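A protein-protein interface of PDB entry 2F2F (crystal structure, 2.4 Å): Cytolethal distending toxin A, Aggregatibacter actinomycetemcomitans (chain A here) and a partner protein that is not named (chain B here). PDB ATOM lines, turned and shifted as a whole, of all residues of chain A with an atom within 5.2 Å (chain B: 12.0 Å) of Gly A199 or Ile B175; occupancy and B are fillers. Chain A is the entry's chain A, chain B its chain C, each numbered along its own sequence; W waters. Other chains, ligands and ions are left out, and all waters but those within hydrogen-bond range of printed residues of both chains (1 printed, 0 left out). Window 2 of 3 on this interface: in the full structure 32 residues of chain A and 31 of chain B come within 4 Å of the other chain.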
ATOM      1  N   LEU A 161       3.348  16.961  13.115  1.00  0.00           N
ATOM      2  CA  LEU A 161       4.682  16.361  13.159  1.00  0.00           C
ATOM      3  C   LEU A 161       5.351  16.545  14.508  1.00  0.00           C
ATOM      4  O   LEU A 161       5.471  17.658  15.010  1.00  0.00           O
ATOM      5  CB  LEU A 161       5.573  16.962  12.070  1.00  0.00           C
ATOM      6  CG  LEU A 161       5.016  17.050  10.647  1.00  0.00           C
ATOM      7  CD1 LEU A 161       6.051  17.666   9.717  1.00  0.00           C
ATOM      8  CD2 LEU A 161       4.661  15.682  10.158  1.00  0.00           C
ATOM      9  N   PRO A 162       5.801  15.443  15.119  1.00  0.00           N
ATOM     10  CA  PRO A 162       6.442  15.619  16.422  1.00  0.00           C
ATOM     11  C   PRO A 162       7.845  16.208  16.272  1.00  0.00           C
ATOM     12  O   PRO A 162       8.462  16.097  15.219  1.00  0.00           O
ATOM     13  CB  PRO A 162       6.457  14.200  16.994  1.00  0.00           C
ATOM     14  CG  PRO A 162       6.566  13.320  15.769  1.00  0.00           C
ATOM     15  CD  PRO A 162       5.827  14.045  14.657  1.00  0.00           C
ATOM     16  N   THR A 163       8.346  16.847  17.321  1.00  0.00           N
ATOM     17  CA  THR A 163       9.695  17.399  17.267  1.00  0.00           C
ATOM     18  C   THR A 163      10.428  16.838  18.479  1.00  0.00           C
ATOM     19  O   THR A 163       9.794  16.299  19.401  1.00  0.00           O
ATOM     20  CB  THR A 163       9.708  18.959  17.353  1.00  0.00           C
ATOM     21  OG1 THR A 163       9.266  19.364  18.651  1.00  0.00           O
ATOM     22  CG2 THR A 163       8.800  19.574  16.296  1.00  0.00           C
ATOM     23  N   ASP A 164      11.749  16.983  18.503  1.00  0.00           N
ATOM     24  CA  ASP A 164      12.500  16.460  19.627  1.00  0.00           C
ATOM     25  C   ASP A 164      12.296  17.198  20.948  1.00  0.00           C
ATOM     26  O   ASP A 164      12.813  16.767  21.972  1.00  0.00           O
ATOM     27  CB  ASP A 164      13.997  16.360  19.289  1.00  0.00           C
ATOM     28  CG  ASP A 164      14.635  17.705  18.967  1.00  0.00           C
ATOM     29  OD1 ASP A 164      14.133  18.766  19.404  1.00  0.00           O
ATOM     30  OD2 ASP A 164      15.662  17.691  18.263  1.00  0.00           O
ATOM     31  N   VAL A 169       4.920  20.705  14.699  1.00  0.00           N
ATOM     32  CA  VAL A 169       5.020  21.525  13.517  1.00  0.00           C
ATOM     33  C   VAL A 169       3.746  21.139  12.771  1.00  0.00           C
ATOM     34  O   VAL A 169       3.464  19.959  12.599  1.00  0.00           O
ATOM     35  CB  VAL A 169       6.271  21.130  12.731  1.00  0.00           C
ATOM     36  CG1 VAL A 169       6.186  21.619  11.326  1.00  0.00           C
ATOM     37  CG2 VAL A 169       7.492  21.685  13.431  1.00  0.00           C
ATOM     38  N   CYS A 197       8.874  23.648   5.327  1.00  0.00           N
ATOM     39  CA  CYS A 197       8.976  23.071   6.660  1.00  0.00           C
ATOM     40  C   CYS A 197      10.428  22.823   7.036  1.00  0.00           C
ATOM     41  O   CYS A 197      11.012  21.824   6.623  1.00  0.00           O
ATOM     42  CB  CYS A 197       8.219  21.747   6.720  1.00  0.00           C
ATOM     43  SG  CYS A 197       6.563  21.852   6.045  1.00  0.00           S
ATOM     44  N   ASP A 198      11.011  23.736   7.807  1.00  0.00           N
ATOM     45  CA  ASP A 198      12.386  23.577   8.246  1.00  0.00           C
ATOM     46  C   ASP A 198      12.511  23.645   9.762  1.00  0.00           C
ATOM     47  O   ASP A 198      13.614  23.719  10.296  1.00  0.00           O
ATOM     48  CB  ASP A 198      13.302  24.610   7.561  1.00  0.00           C
ATOM     49  CG  ASP A 198      12.876  26.046   7.802  1.00  0.00           C
ATOM     50  OD1 ASP A 198      12.415  26.356   8.920  1.00  0.00           O
ATOM     51  OD2 ASP A 198      13.011  26.868   6.864  1.00  0.00           O
ATOM     52  N   GLY A 199      11.379  23.596  10.457  1.00  0.00           N
ATOM     53  CA  GLY A 199      11.410  23.648  11.912  1.00  0.00           C
ATOM     54  C   GLY A 199      12.203  24.817  12.481  1.00  0.00           C
ATOM     55  O   GLY A 199      12.833  24.704  13.527  1.00  0.00           O
ATOM     56  N   ALA A 200      12.176  25.941  11.773  1.00  0.00           N
ATOM     57  CA  ALA A 200      12.876  27.143  12.198  1.00  0.00           C
ATOM     58  C   ALA A 200      12.288  27.686  13.487  1.00  0.00           C
ATOM     59  O   ALA A 200      11.091  27.575  13.719  1.00  0.00           O
ATOM     60  CB  ALA A 200      12.781  28.201  11.113  1.00  0.00           C
ATOM     61  N   THR A 201      13.139  28.217  14.351  1.00  0.00           N
ATOM     62  CA  THR A 201      12.670  28.837  15.571  1.00  0.00           C
ATOM     63  C   THR A 201      13.432  30.157  15.708  1.00  0.00           C
ATOM     64  O   THR A 201      14.352  30.261  16.524  1.00  0.00           O
ATOM     65  CB  THR A 201      12.929  27.939  16.808  1.00  0.00           C
ATOM     66  OG1 THR A 201      14.295  27.515  16.831  1.00  0.00           O
ATOM     67  CG2 THR A 201      12.050  26.704  16.749  1.00  0.00           C
ATOM     68  N   GLN A 207       8.115  27.897  13.525  1.00  0.00           N
ATOM     69  CA  GLN A 207       7.159  26.913  13.044  1.00  0.00           C
ATOM     70  C   GLN A 207       6.679  25.935  14.106  1.00  0.00           C
ATOM     71  O   GLN A 207       5.992  24.970  13.787  1.00  0.00           O
ATOM     72  CB  GLN A 207       7.734  26.149  11.854  1.00  0.00           C
ATOM     73  CG  GLN A 207       7.858  27.003  10.636  1.00  0.00           C
ATOM     74  CD  GLN A 207       8.431  26.259   9.485  1.00  0.00           C
ATOM     75  OE1 GLN A 207       9.050  25.218   9.663  1.00  0.00           O
ATOM     76  NE2 GLN A 207       8.232  26.773   8.288  1.00  0.00           N
ATOM     77  N   THR A 208       7.058  26.159  15.361  1.00  0.00           N
ATOM     78  CA  THR A 208       6.651  25.267  16.433  1.00  0.00           C
ATOM     79  C   THR A 208       5.508  25.760  17.325  1.00  0.00           C
ATOM     80  O   THR A 208       5.465  26.909  17.754  1.00  0.00           O
ATOM     81  CB  THR A 208       7.905  24.824  17.286  1.00  0.00           C
ATOM     82  OG1 THR A 208       8.207  25.797  18.277  1.00  0.00           O
ATOM     83  CG2 THR A 208       9.137  24.681  16.397  1.00  0.00           C
ATOM     84  N   TYR B  61      17.277  30.740  26.509  1.00  0.00           N
ATOM     85  CA  TYR B  61      16.037  29.965  26.556  1.00  0.00           C
ATOM     86  C   TYR B  61      16.071  28.949  27.690  1.00  0.00           C
ATOM     87  O   TYR B  61      15.032  28.631  28.259  1.00  0.00           O
ATOM     88  CB  TYR B  61      15.778  29.251  25.225  1.00  0.00           C
ATOM     89  CG  TYR B  61      16.798  28.208  24.814  1.00  0.00           C
ATOM     90  CD1 TYR B  61      16.788  26.935  25.368  1.00  0.00           C
ATOM     91  CD2 TYR B  61      17.730  28.480  23.822  1.00  0.00           C
ATOM     92  CE1 TYR B  61      17.675  25.958  24.940  1.00  0.00           C
ATOM     93  CE2 TYR B  61      18.619  27.514  23.388  1.00  0.00           C
ATOM     94  CZ  TYR B  61      18.588  26.250  23.948  1.00  0.00           C
ATOM     95  OH  TYR B  61      19.464  25.275  23.510  1.00  0.00           O
ATOM     96  N   PRO B 169       9.533  22.467  26.492  1.00  0.00           N
ATOM     97  CA  PRO B 169      10.507  23.498  26.850  1.00  0.00           C
ATOM     98  C   PRO B 169      10.715  24.516  25.727  1.00  0.00           C
ATOM     99  O   PRO B 169      11.047  24.156  24.590  1.00  0.00           O
ATOM    100  CB  PRO B 169      11.767  22.690  27.180  1.00  0.00           C
ATOM    101  CG  PRO B 169      11.627  21.462  26.401  1.00  0.00           C
ATOM    102  CD  PRO B 169      10.160  21.138  26.419  1.00  0.00           C
ATOM    103  N   PHE B 170      10.528  25.790  26.071  1.00  0.00           N
ATOM    104  CA  PHE B 170      10.686  26.902  25.134  1.00  0.00           C
ATOM    105  C   PHE B 170      12.066  26.901  24.493  1.00  0.00           C
ATOM    106  O   PHE B 170      13.064  26.715  25.163  1.00  0.00           O
ATOM    107  CB  PHE B 170      10.471  28.242  25.862  1.00  0.00           C
ATOM    108  CG  PHE B 170      10.880  29.443  25.054  1.00  0.00           C
ATOM    109  CD1 PHE B 170      10.075  29.901  24.017  1.00  0.00           C
ATOM    110  CD2 PHE B 170      12.119  30.061  25.265  1.00  0.00           C
ATOM    111  CE1 PHE B 170      10.501  30.951  23.186  1.00  0.00           C
ATOM    112  CE2 PHE B 170      12.555  31.110  24.444  1.00  0.00           C
ATOM    113  CZ  PHE B 170      11.744  31.553  23.400  1.00  0.00           C
ATOM    114  N   GLY B 171      12.129  27.109  23.193  1.00  0.00           N
ATOM    115  CA  GLY B 171      13.421  27.122  22.559  1.00  0.00           C
ATOM    116  C   GLY B 171      13.396  26.462  21.209  1.00  0.00           C
ATOM    117  O   GLY B 171      12.356  26.368  20.572  1.00  0.00           O
ATOM    118  N   PRO B 172      14.544  25.980  20.752  1.00  0.00           N
ATOM    119  CA  PRO B 172      14.671  25.316  19.459  1.00  0.00           C
ATOM    120  C   PRO B 172      14.235  23.854  19.546  1.00  0.00           C
ATOM    121  O   PRO B 172      14.082  23.296  20.637  1.00  0.00           O
ATOM    122  CB  PRO B 172      16.152  25.452  19.142  1.00  0.00           C
ATOM    123  CG  PRO B 172      16.806  25.432  20.486  1.00  0.00           C
ATOM    124  CD  PRO B 172      15.816  25.995  21.493  1.00  0.00           C
ATOM    125  N   SER B 173      14.022  23.243  18.391  1.00  0.00           N
ATOM    126  CA  SER B 173      13.615  21.854  18.341  1.00  0.00           C
ATOM    127  C   SER B 173      13.782  21.420  16.917  1.00  0.00           C
ATOM    128  O   SER B 173      13.871  22.248  16.017  1.00  0.00           O
ATOM    129  CB  SER B 173      12.173  21.696  18.791  1.00  0.00           C
ATOM    130  OG  SER B 173      11.338  22.414  17.932  1.00  0.00           O
ATOM    131  N   LYS B 174      13.893  20.115  16.726  1.00  0.00           N
ATOM    132  CA  LYS B 174      14.071  19.539  15.402  1.00  0.00           C
ATOM    133  C   LYS B 174      12.916  18.605  15.070  1.00  0.00           C
ATOM    134  O   LYS B 174      12.425  17.884  15.941  1.00  0.00           O
ATOM    135  CB  LYS B 174      15.399  18.786  15.366  1.00  0.00           C
ATOM    136  CG  LYS B 174      15.723  18.146  14.027  1.00  0.00           C
ATOM    137  CD  LYS B 174      16.940  17.194  14.105  1.00  0.00           C
ATOM    138  CE  LYS B 174      16.562  15.781  14.603  1.00  0.00           C
ATOM    139  NZ  LYS B 174      15.765  14.977  13.621  1.00  0.00           N
ATOM    140  N   ILE B 175      12.453  18.645  13.826  1.00  0.00           N
ATOM    141  CA  ILE B 175      11.363  17.770  13.397  1.00  0.00           C
ATOM    142  C   ILE B 175      11.894  16.341  13.397  1.00  0.00           C
ATOM    143  O   ILE B 175      12.949  16.075  12.821  1.00  0.00           O
ATOM    144  CB  ILE B 175      10.872  18.112  11.944  1.00  0.00           C
ATOM    145  CG1 ILE B 175      10.236  19.506  11.912  1.00  0.00           C
ATOM    146  CG2 ILE B 175       9.825  17.089  11.472  1.00  0.00           C
ATOM    147  CD1 ILE B 175      10.004  20.038  10.519  1.00  0.00           C
ATOM    148  N   LEU B 176      11.157  15.419  14.012  1.00  0.00           N
ATOM    149  CA  LEU B 176      11.588  14.027  14.043  1.00  0.00           C
ATOM    150  C   LEU B 176      11.162  13.356  12.743  1.00  0.00           C
ATOM    151  O   LEU B 176       9.983  13.338  12.381  1.00  0.00           O
ATOM    152  CB  LEU B 176      10.973  13.279  15.225  1.00  0.00           C
ATOM    153  CG  LEU B 176      11.448  13.734  16.588  1.00  0.00           C
ATOM    154  CD1 LEU B 176      10.831  12.878  17.640  1.00  0.00           C
ATOM    155  CD2 LEU B 176      12.943  13.657  16.646  1.00  0.00           C
ATOM    156  N   ARG B 177      12.148  12.780  12.069  1.00  0.00           N
ATOM    157  CA  ARG B 177      11.965  12.108  10.794  1.00  0.00           C
ATOM    158  C   ARG B 177      12.113  10.589  10.998  1.00  0.00           C
ATOM    159  O   ARG B 177      13.045  10.145  11.664  1.00  0.00           O
ATOM    160  CB  ARG B 177      13.028  12.630   9.836  1.00  0.00           C
ATOM    161  CG  ARG B 177      12.501  13.136   8.509  1.00  0.00           C
ATOM    162  CD  ARG B 177      11.456  14.245   8.532  1.00  0.00           C
ATOM    163  NE  ARG B 177      10.118  14.064   9.159  1.00  0.00           N
ATOM    164  CZ  ARG B 177       9.153  13.209   8.818  1.00  0.00           C
ATOM    165  NH1 ARG B 177       9.233  12.352   7.835  1.00  0.00           N
ATOM    166  NH2 ARG B 177       7.951  13.373   9.278  1.00  0.00           N
ATOM    167  N   PRO B 178      11.192   9.776  10.423  1.00  0.00           N
ATOM    168  CA  PRO B 178      11.263   8.312  10.578  1.00  0.00           C
ATOM    169  C   PRO B 178      12.361   7.641   9.771  1.00  0.00           C
ATOM    170  O   PRO B 178      12.893   8.302   8.855  1.00  0.00           O
ATOM    171  CB  PRO B 178       9.872   7.835  10.164  1.00  0.00           C
ATOM    172  CG  PRO B 178       9.399   8.868   9.196  1.00  0.00           C
ATOM    173  CD  PRO B 178      10.048  10.178   9.584  1.00  0.00           C
HETATM  174  O   HOH W   1      10.457  24.593  19.861  1.00  0.00           O
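O of Pro A162 lies within hydrogen-bond range of N of Leu B176 (3.0 Å). The backbone NH (N) of Asp A164 sits at hydrogen-bond distance from the backbone carbonyl oxygen (O) of Lys B174 (2.8 Å).
N of Leu A161 lies within hydrogen-bond range of O of Val A169 (3.0 Å). N of Gly A199 lies within hydrogen-bond range of OE1 of Gln A207 (2.9 Å).
Among the printed residues, merely in contact across the chains: Pro A162 with Ile B175, Thr A163 with Ser B173, Thr A163 with Lys B174, Thr A163 with Leu B176, Asp A164 with Ser B173, Asp A164 with Leu B176, Val A169 with Ile B175, Gly A199 with Ser B173, Gly A199 with Ile B175, Thr A201 with Gly B171, Thr A201 with Pro B172 and Thr A208 with Ser B173.
Of chain B, only Ile B175 and Leu B176 come within 4 Å of Pro A162. Of chain B, only Ser B173 (3.7 Å), Lys B174 (3.1 Å) and Leu B176 (3.8 Å) come within 4 Å of Thr A163. Of the printed residues of chain B, Asp A164 touches Ser B173 (3.3 Å), Lys B174 (2.8 Å) and Leu B176 (3.8 Å). No residue of chain B comes within 4 Å of Cys A197. No residue of chain B comes within 4 Å of Asp A198. Of chain B, only Ser B173 and Ile B175 come within 4 Å of Gly A199. No residue of chain B comes within 4 Å of Ala A200. Tyr B61 touches none of the printed residues of chain A. Of the printed residues of chain A, Ser B173 touches Thr A163 (3.7 Å), Asp A164 (3.3 Å), Gly A199 (3.6 Å) and Thr A208 (3.5 Å). Printed residues of chain A within 4 Å of Ile B175: Pro A162, Val A169 and Gly A199. The nearest residue of chain B that does not touch Gly A199 is Lys B174 (5.6 Å). The nearest printed residue of chain A that does not touch Ile B175 is Leu A161 (4.2 Å).
Among the printed residues, 14 pairs touch across the chains.
Water W1 lies within hydrogen-bond range of the backbone carbonyl oxygen (O) of Gly B171, the side-chain hydroxyl (OG1) of Thr A208 and the side-chain hydroxyl (OG) of Ser B173.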
